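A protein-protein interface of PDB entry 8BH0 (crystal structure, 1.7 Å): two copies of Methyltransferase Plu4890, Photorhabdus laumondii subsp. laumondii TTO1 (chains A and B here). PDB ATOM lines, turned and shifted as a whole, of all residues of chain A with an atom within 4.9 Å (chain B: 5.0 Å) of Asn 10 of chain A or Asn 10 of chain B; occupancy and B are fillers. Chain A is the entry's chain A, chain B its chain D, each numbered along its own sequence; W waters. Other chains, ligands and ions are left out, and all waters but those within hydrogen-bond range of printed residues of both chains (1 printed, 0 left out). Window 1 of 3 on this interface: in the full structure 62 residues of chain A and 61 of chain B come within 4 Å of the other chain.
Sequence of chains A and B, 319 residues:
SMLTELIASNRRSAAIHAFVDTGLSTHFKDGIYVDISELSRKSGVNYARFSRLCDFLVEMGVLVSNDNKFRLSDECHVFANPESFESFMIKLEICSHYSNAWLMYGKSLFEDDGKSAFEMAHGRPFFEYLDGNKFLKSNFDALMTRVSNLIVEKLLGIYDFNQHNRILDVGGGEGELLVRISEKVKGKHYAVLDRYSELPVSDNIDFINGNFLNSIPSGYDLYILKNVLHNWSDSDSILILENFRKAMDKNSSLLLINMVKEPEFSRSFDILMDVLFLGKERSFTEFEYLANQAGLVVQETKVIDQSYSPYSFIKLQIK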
ATOM      1  N   ILE A   7       5.205  22.070   3.870  1.00  0.00           N
ATOM      2  CA  ILE A   7       5.134  20.807   4.667  1.00  0.00           C
ATOM      3  C   ILE A   7       6.532  20.173   4.700  1.00  0.00           C
ATOM      4  O   ILE A   7       6.917  19.641   5.762  1.00  0.00           O
ATOM      5  CB  ILE A   7       4.067  19.846   4.100  1.00  0.00           C
ATOM      6  CG1 ILE A   7       2.652  20.400   4.297  1.00  0.00           C
ATOM      7  CG2 ILE A   7       4.214  18.456   4.703  1.00  0.00           C
ATOM      8  CD1 ILE A   7       1.576  19.629   3.562  1.00  0.00           C
ATOM      9  N   ALA A   8       7.269  20.259   3.588  1.00  0.00           N
ATOM     10  CA  ALA A   8       8.601  19.641   3.386  1.00  0.00           C
ATOM     11  C   ALA A   8       9.728  20.595   3.813  1.00  0.00           C
ATOM     12  O   ALA A   8      10.873  20.360   3.390  1.00  0.00           O
ATOM     13  CB  ALA A   8       8.752  19.238   1.939  1.00  0.00           C
ATOM     14  N   SER A   9       9.432  21.615   4.627  1.00  0.00           N
ATOM     15  CA  SER A   9      10.432  22.593   5.137  1.00  0.00           C
ATOM     16  C   SER A   9      11.602  21.851   5.800  1.00  0.00           C
ATOM     17  O   SER A   9      12.754  22.285   5.610  1.00  0.00           O
ATOM     18  CB  SER A   9       9.805  23.585   6.080  1.00  0.00           C
ATOM     19  OG  SER A   9       8.945  24.474   5.385  1.00  0.00           O
ATOM     20  N   ASN A  10      11.314  20.770   6.534  1.00  0.00           N
ATOM     21  CA  ASN A  10      12.314  19.929   7.250  1.00  0.00           C
ATOM     22  C   ASN A  10      13.453  19.513   6.307  1.00  0.00           C
ATOM     23  O   ASN A  10      14.588  19.392   6.787  1.00  0.00           O
ATOM     24  CB  ASN A  10      11.676  18.677   7.857  1.00  0.00           C
ATOM     25  CG  ASN A  10      11.057  17.788   6.801  1.00  0.00           C
ATOM     26  OD1 ASN A  10      10.277  18.264   5.979  1.00  0.00           O
ATOM     27  ND2 ASN A  10      11.412  16.512   6.795  1.00  0.00           N
ATOM     28  N   ARG A  11      13.161  19.296   5.021  1.00  0.00           N
ATOM     29  CA  ARG A  11      14.157  18.820   4.020  1.00  0.00           C
ATOM     30  C   ARG A  11      15.277  19.858   3.868  1.00  0.00           C
ATOM     31  O   ARG A  11      16.423  19.444   3.625  1.00  0.00           O
ATOM     32  CB  ARG A  11      13.482  18.520   2.679  1.00  0.00           C
ATOM     33  CG  ARG A  11      12.406  17.450   2.774  1.00  0.00           C
ATOM     34  CD  ARG A  11      11.821  17.086   1.426  1.00  0.00           C
ATOM     35  NE  ARG A  11      10.557  16.382   1.582  1.00  0.00           N
ATOM     36  CZ  ARG A  11       9.669  16.183   0.614  1.00  0.00           C
ATOM     37  NH1 ARG A  11       8.543  15.542   0.880  1.00  0.00           N
ATOM     38  NH2 ARG A  11       9.897  16.626  -0.612  1.00  0.00           N
ATOM     39  N   ARG A  12      14.964  21.150   4.019  1.00  0.00           N
ATOM     40  CA  ARG A  12      15.969  22.244   3.913  1.00  0.00           C
ATOM     41  C   ARG A  12      16.971  22.100   5.063  1.00  0.00           C
ATOM     42  O   ARG A  12      18.186  22.116   4.791  1.00  0.00           O
ATOM     43  CB  ARG A  12      15.310  23.628   3.926  1.00  0.00           C
ATOM     44  CG  ARG A  12      14.699  24.042   2.595  1.00  0.00           C
ATOM     45  CD  ARG A  12      13.413  23.306   2.283  1.00  0.00           C
ATOM     46  NE  ARG A  12      12.861  23.687   0.991  1.00  0.00           N
ATOM     47  CZ  ARG A  12      11.888  23.037   0.359  1.00  0.00           C
ATOM     48  NH1 ARG A  12      11.464  23.472  -0.816  1.00  0.00           N
ATOM     49  NH2 ARG A  12      11.342  21.955   0.894  1.00  0.00           N
ATOM     50  N   SER A  13      16.470  21.961   6.293  1.00  0.00           N
ATOM     51  CA  SER A  13      17.282  21.782   7.526  1.00  0.00           C
ATOM     52  C   SER A  13      18.136  20.513   7.405  1.00  0.00           C
ATOM     53  O   SER A  13      19.331  20.566   7.740  1.00  0.00           O
ATOM     54  CB  SER A  13      16.405  21.746   8.753  1.00  0.00           C
ATOM     55  OG  SER A  13      15.798  23.011   8.975  1.00  0.00           O
ATOM     56  N   ALA A  14      17.548  19.414   6.923  1.00  0.00           N
ATOM     57  CA  ALA A  14      18.218  18.096   6.823  1.00  0.00           C
ATOM     58  C   ALA A  14      19.326  18.147   5.763  1.00  0.00           C
ATOM     59  O   ALA A  14      20.394  17.539   5.995  1.00  0.00           O
ATOM     60  CB  ALA A  14      17.204  17.019   6.532  1.00  0.00           C
ATOM     61  N   GLU A  93      19.635  21.333  15.739  1.00  0.00           N
ATOM     62  CA  GLU A  93      18.306  21.697  15.173  1.00  0.00           C
ATOM     63  C   GLU A  93      17.505  20.431  14.833  1.00  0.00           C
ATOM     64  O   GLU A  93      16.329  20.374  15.230  1.00  0.00           O
ATOM     65  CB  GLU A  93      18.460  22.604  13.950  1.00  0.00           C
ATOM     66  CG  GLU A  93      17.156  23.241  13.506  1.00  0.00           C
ATOM     67  CD  GLU A  93      16.511  24.198  14.498  1.00  0.00           C
ATOM     68  OE1 GLU A  93      17.247  24.844  15.270  1.00  0.00           O
ATOM     69  OE2 GLU A  93      15.266  24.297  14.498  1.00  0.00           O
ATOM     70  N   ILE A  94      18.102  19.457  14.134  1.00  0.00           N
ATOM     71  CA  ILE A  94      17.387  18.216  13.697  1.00  0.00           C
ATOM     72  C   ILE A  94      17.994  16.975  14.365  1.00  0.00           C
ATOM     73  O   ILE A  94      17.765  15.864  13.844  1.00  0.00           O
ATOM     74  CB  ILE A  94      17.365  18.077  12.161  1.00  0.00           C
ATOM     75  CG1 ILE A  94      18.755  17.842  11.563  1.00  0.00           C
ATOM     76  CG2 ILE A  94      16.669  19.271  11.526  1.00  0.00           C
ATOM     77  CD1 ILE A  94      18.733  16.957  10.340  1.00  0.00           C
ATOM     78  N   TRP A 102       9.870  17.632  19.346  1.00  0.00           N
ATOM     79  CA  TRP A 102       8.904  18.195  18.363  1.00  0.00           C
ATOM     80  C   TRP A 102       7.724  17.236  18.175  1.00  0.00           C
ATOM     81  O   TRP A 102       6.597  17.724  18.013  1.00  0.00           O
ATOM     82  CB  TRP A 102       9.584  18.510  17.024  1.00  0.00           C
ATOM     83  CG  TRP A 102      10.321  19.813  17.011  1.00  0.00           C
ATOM     84  CD1 TRP A 102      11.670  19.994  16.924  1.00  0.00           C
ATOM     85  CD2 TRP A 102       9.746  21.129  17.099  1.00  0.00           C
ATOM     86  NE1 TRP A 102      11.972  21.328  16.941  1.00  0.00           N
ATOM     87  CE2 TRP A 102      10.813  22.049  17.045  1.00  0.00           C
ATOM     88  CE3 TRP A 102       8.439  21.619  17.205  1.00  0.00           C
ATOM     89  CZ2 TRP A 102      10.611  23.428  17.102  1.00  0.00           C
ATOM     90  CZ3 TRP A 102       8.239  22.982  17.245  1.00  0.00           C
ATOM     91  CH2 TRP A 102       9.313  23.871  17.203  1.00  0.00           C
ATOM     92  N   ILE B   7      18.133  27.611   8.481  1.00  0.00           N
ATOM     93  CA  ILE B   7      18.635  26.501   9.347  1.00  0.00           C
ATOM     94  C   ILE B   7      17.445  25.917  10.121  1.00  0.00           C
ATOM     95  O   ILE B   7      17.380  24.678  10.250  1.00  0.00           O
ATOM     96  CB  ILE B   7      19.772  26.985  10.274  1.00  0.00           C
ATOM     97  CG1 ILE B   7      21.036  27.322   9.479  1.00  0.00           C
ATOM     98  CG2 ILE B   7      20.055  25.966  11.369  1.00  0.00           C
ATOM     99  CD1 ILE B   7      22.085  28.071  10.272  1.00  0.00           C
ATOM    100  N   ALA B   8      16.523  26.777  10.569  1.00  0.00           N
ATOM    101  CA  ALA B   8      15.361  26.436  11.427  1.00  0.00           C
ATOM    102  C   ALA B   8      14.118  26.117  10.581  1.00  0.00           C
ATOM    103  O   ALA B   8      13.004  26.184  11.135  1.00  0.00           O
ATOM    104  CB  ALA B   8      15.093  27.573  12.383  1.00  0.00           C
ATOM    105  N   SER B   9      14.289  25.760   9.303  1.00  0.00           N
ATOM    106  CA  SER B   9      13.182  25.374   8.384  1.00  0.00           C
ATOM    107  C   SER B   9      12.331  24.265   9.017  1.00  0.00           C
ATOM    108  O   SER B   9      11.098  24.309   8.864  1.00  0.00           O
ATOM    109  CB  SER B   9      13.707  24.960   7.034  1.00  0.00           C
ATOM    110  OG  SER B   9      14.301  26.060   6.360  1.00  0.00           O
ATOM    111  N   ASN B  10      12.967  23.320   9.717  1.00  0.00           N
ATOM    112  CA  ASN B  10      12.308  22.167  10.397  1.00  0.00           C
ATOM    113  C   ASN B  10      11.153  22.644  11.290  1.00  0.00           C
ATOM    114  O   ASN B  10      10.163  21.904  11.405  1.00  0.00           O
ATOM    115  CB  ASN B  10      13.303  21.362  11.235  1.00  0.00           C
ATOM    116  CG  ASN B  10      13.928  22.196  12.333  1.00  0.00           C
ATOM    117  OD1 ASN B  10      14.448  23.277  12.063  1.00  0.00           O
ATOM    118  ND2 ASN B  10      13.866  21.724  13.567  1.00  0.00           N
ATOM    119  N   ARG B  11      11.270  23.825  11.907  1.00  0.00           N
ATOM    120  CA  ARG B  11      10.264  24.348  12.873  1.00  0.00           C
ATOM    121  C   ARG B  11       8.921  24.563  12.166  1.00  0.00           C
ATOM    122  O   ARG B  11       7.885  24.427  12.834  1.00  0.00           O
ATOM    123  CB  ARG B  11      10.755  25.642  13.527  1.00  0.00           C
ATOM    124  CG  ARG B  11      12.055  25.467  14.294  1.00  0.00           C
ATOM    125  CD  ARG B  11      12.500  26.727  14.996  1.00  0.00           C
ATOM    126  NE  ARG B  11      13.900  26.629  15.374  1.00  0.00           N
ATOM    127  CZ  ARG B  11      14.662  27.655  15.737  1.00  0.00           C
ATOM    128  NH1 ARG B  11      15.933  27.451  16.042  1.00  0.00           N
ATOM    129  NH2 ARG B  11      14.159  28.878  15.785  1.00  0.00           N
ATOM    130  N   ARG B  12       8.939  24.880  10.867  1.00  0.00           N
ATOM    131  CA  ARG B  12       7.709  25.095  10.056  1.00  0.00           C
ATOM    132  C   ARG B  12       6.970  23.757   9.917  1.00  0.00           C
ATOM    133  O   ARG B  12       5.748  23.732  10.155  1.00  0.00           O
ATOM    134  CB  ARG B  12       8.042  25.697   8.688  1.00  0.00           C
ATOM    135  CG  ARG B  12       8.323  27.193   8.712  1.00  0.00           C
ATOM    136  CD  ARG B  12       9.690  27.563   9.255  1.00  0.00           C
ATOM    137  NE  ARG B  12       9.850  29.008   9.352  1.00  0.00           N
ATOM    138  CZ  ARG B  12      10.811  29.627  10.033  1.00  0.00           C
ATOM    139  NH1 ARG B  12      10.854  30.949  10.051  1.00  0.00           N
ATOM    140  NH2 ARG B  12      11.723  28.934  10.696  1.00  0.00           N
ATOM    141  N   SER B  13       7.686  22.689   9.556  1.00  0.00           N
ATOM    142  CA  SER B  13       7.129  21.315   9.422  1.00  0.00           C
ATOM    143  C   SER B  13       6.583  20.856  10.778  1.00  0.00           C
ATOM    144  O   SER B  13       5.462  20.320  10.817  1.00  0.00           O
ATOM    145  CB  SER B  13       8.158  20.351   8.890  1.00  0.00           C
ATOM    146  OG  SER B  13       8.557  20.708   7.575  1.00  0.00           O
ATOM    147  N   ALA B  14       7.345  21.083  11.852  1.00  0.00           N
ATOM    148  CA  ALA B  14       7.007  20.651  13.229  1.00  0.00           C
ATOM    149  C   ALA B  14       5.745  21.379  13.711  1.00  0.00           C
ATOM    150  O   ALA B  14       4.893  20.731  14.350  1.00  0.00           O
ATOM    151  CB  ALA B  14       8.178  20.887  14.151  1.00  0.00           C
ATOM    152  N   GLU B  93       6.334  12.985   7.203  1.00  0.00           N
ATOM    153  CA  GLU B  93       7.460  13.905   6.874  1.00  0.00           C
ATOM    154  C   GLU B  93       8.465  13.991   8.032  1.00  0.00           C
ATOM    155  O   GLU B  93       9.681  13.927   7.749  1.00  0.00           O
ATOM    156  CB  GLU B  93       6.931  15.297   6.513  1.00  0.00           C
ATOM    157  CG  GLU B  93       7.986  16.209   5.912  1.00  0.00           C
ATOM    158  CD  GLU B  93       8.514  15.788   4.548  1.00  0.00           C
ATOM    159  OE1 GLU B  93       7.726  15.240   3.749  1.00  0.00           O
ATOM    160  OE2 GLU B  93       9.715  16.011   4.283  1.00  0.00           O
ATOM    161  N   ILE B  94       7.998  14.152   9.277  1.00  0.00           N
ATOM    162  CA  ILE B  94       8.893  14.349  10.460  1.00  0.00           C
ATOM    163  C   ILE B  94       8.700  13.217  11.477  1.00  0.00           C
ATOM    164  O   ILE B  94       9.115  13.403  12.638  1.00  0.00           O
ATOM    165  CB  ILE B  94       8.686  15.739  11.101  1.00  0.00           C
ATOM    166  CG1 ILE B  94       7.323  15.876  11.783  1.00  0.00           C
ATOM    167  CG2 ILE B  94       8.919  16.843  10.081  1.00  0.00           C
ATOM    168  CD1 ILE B  94       7.328  16.844  12.941  1.00  0.00           C
ATOM    169  N   TRP B 102      17.129  10.793   7.781  1.00  0.00           N
ATOM    170  CA  TRP B 102      17.774  12.096   7.460  1.00  0.00           C
ATOM    171  C   TRP B 102      19.104  12.235   8.215  1.00  0.00           C
ATOM    172  O   TRP B 102      20.053  12.797   7.633  1.00  0.00           O
ATOM    173  CB  TRP B 102      16.834  13.272   7.753  1.00  0.00           C
ATOM    174  CG  TRP B 102      15.845  13.548   6.663  1.00  0.00           C
ATOM    175  CD1 TRP B 102      14.493  13.371   6.713  1.00  0.00           C
ATOM    176  CD2 TRP B 102      16.134  14.046   5.345  1.00  0.00           C
ATOM    177  NE1 TRP B 102      13.921  13.730   5.523  1.00  0.00           N
ATOM    178  CE2 TRP B 102      14.902  14.148   4.663  1.00  0.00           C
ATOM    179  CE3 TRP B 102      17.306  14.420   4.676  1.00  0.00           C
ATOM    180  CZ2 TRP B 102      14.814  14.607   3.350  1.00  0.00           C
ATOM    181  CZ3 TRP B 102      17.217  14.879   3.381  1.00  0.00           C
ATOM    182  CH2 TRP B 102      15.987  14.967   2.728  1.00  0.00           C
HETATM  183  O   HOH W   1      14.712  22.221  16.123  1.00  0.00           O
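NE of Arg 11 of chain A is in salt-bridge range of OE2 of Glu 93 of chain B, 2.9 Å away.
NE of Arg 11 of chain B is in salt-bridge range of OE2 of Glu 93 of chain A, 2.8 Å away.
The backbone carbonyl oxygen (O) of Ile 7 of chain A is in hydrogen-bond range of the side-chain hydroxyl (OG) of Ser 13 of chain B (2.7 Å).
OG of Ser 13 of chain A sits at hydrogen-bond distance from O of Ile 7 of chain B, 2.6 Å away.
N of Ser 9 of chain A is in hydrogen-bond range of OG of Ser 13 of chain B (3.2 Å).
N of Ser 9 of chain B sits at hydrogen-bond distance from OG of Ser 13 of chain A (3.2 Å).
The side-chain carboxylate (OE2) of Glu 93 of chain B sits close to the side-chain amide oxygen (OD1) of Asn 10 of chain A, at 2.9 Å.
The side-chain amide oxygen (OD1) of Asn 10 of chain B lies close to the side-chain carboxylate (OE2) of Glu 93 of chain A, at 2.8 Å.
The side-chain hydroxyl of Ser 13 of chain A is in hydrogen-bond range of the backbone NH of Asn 10 of chain B (2.9 Å).
N of Asn 10 of chain A lies within hydrogen-bond range of OG of Ser 13 of chain B (2.9 Å).
The backbone carbonyl oxygen (O) of Ala 8 of chain A lies close to the side-chain amide oxygen (OD1) of Asn 10 of chain A, 3.4 Å away.
The backbone carbonyl oxygen of Ala 8 of chain A lies within hydrogen-bond range of the guanidinium group of Arg 12 of chain A (3.0 Å).
The backbone carbonyl oxygen (O) of Ala 8 of chain B lies within hydrogen-bond range of the guanidinium group (NH2) of Arg 12 of chain B, 3.1 Å away.
O of Ala 8 of chain B lies close to OD1 of Asn 10 of chain B (3.4 Å).
Glu 93 of chain B touches Ile 7 of chain A.
Ser 9 of chain B touches Ser 9 of chain A.
Asn 10 of chain A touches Asn 10 of chain B (CA to CA, 3.9 Å).
CB of Asn 10 of chain A touches CG2 of Ile 94 of chain B, 3.99 Å away.
Ser 13 of chain A touches Ala 8 of chain B (OG to C, 3.9 Å).
O of Ile 7 of chain B touches CG of Glu 93 of chain A, 3.6 Å away.
Glu 93 of chain A touches Ala 8 of chain B.
Ile 94 of chain A touches Asn 10 of chain B.
Trp 102 of chain A touches Arg 11 of chain B.
Trp 102 of chain A touches Ala 14 of chain B.
Of the printed residues of chain B, Ile 7 of chain A touches Ser 13 (2.7 Å) and Glu 93 (3.6 Å).
Printed residues of chain B within 4 Å of Ser 9 of chain A: Ser 9 (3.2 Å), Arg 12 (3.6 Å) and Ser 13 (3.2 Å).
Of the printed residues of chain B, Asn 10 of chain A touches Asn 10 (3.9 Å), Ser 13 (2.9 Å), Glu 93 (2.9 Å), Ile 94 (3.99 Å) and Trp 102 (3.96 Å).
Printed residues of chain B within 4 Å of Trp 102 of chain A: Asn 10 (3.9 Å), Arg 11 (3.8 Å) and Ala 14 (3.2 Å).
Of the printed residues of chain A, Asn 10 of chain B touches Asn 10, Ser 13, Glu 93, Ile 94 and Trp 102.
The nearest printed residue of chain B that does not touch Asn 10 of chain A is Ser 9 of chain B (4.2 Å).
The nearest residue of chain A that does not touch Asn 10 of chain B is Ser 9 of chain A (4.2 Å).
The nearest printed residue of chain B that does not touch Ser 9 of chain A is Asn 10 of chain B (4.2 Å).
Printed residues of chain B that touch a printed residue of chain A: Ile 7, Ala 8, Ser 9, Asn 10, Arg 11, Arg 12, Ser 13, Ala 14, Glu 93, Ile 94 and Trp 102.
Hydrophobic or aromatic side chains of chain A within 4 Å of the printed part of chain B: Ala 14, Ile 94 and Trp 102.
Among the printed residues, Asp or Glu carboxylates within 4 Å of a Lys or Arg side-chain nitrogen of the other chain: Arg 11 of chain A with Glu 93 of chain B (2.9 Å) and Glu 93 of chain A with Arg 11 of chain B (2.8 Å).
Ala 8 of chain A touches Ser 13 of chain B, and with the chains exchanged Ser 13 of chain A touches Ala 8 of chain B.
Ala 8 of chain A touches Glu 93 of chain B, and with the chains exchanged Glu 93 of chain A touches Ala 8 of chain B.
Asn 10 of chain A touches Ser 13 of chain B, and with the chains exchanged Ser 13 of chain A touches Asn 10 of chain B.
Asn 10 of chain A touches Trp 102 of chain B, and with the chains exchanged Trp 102 of chain A touches Asn 10 of chain B.
11 positions are printed for both chains.
Water W1 lies within hydrogen-bond range of O of Glu 93 of chain A, ND2 of Asn 10 of chain B and NE1 of Trp 102 of chain A.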
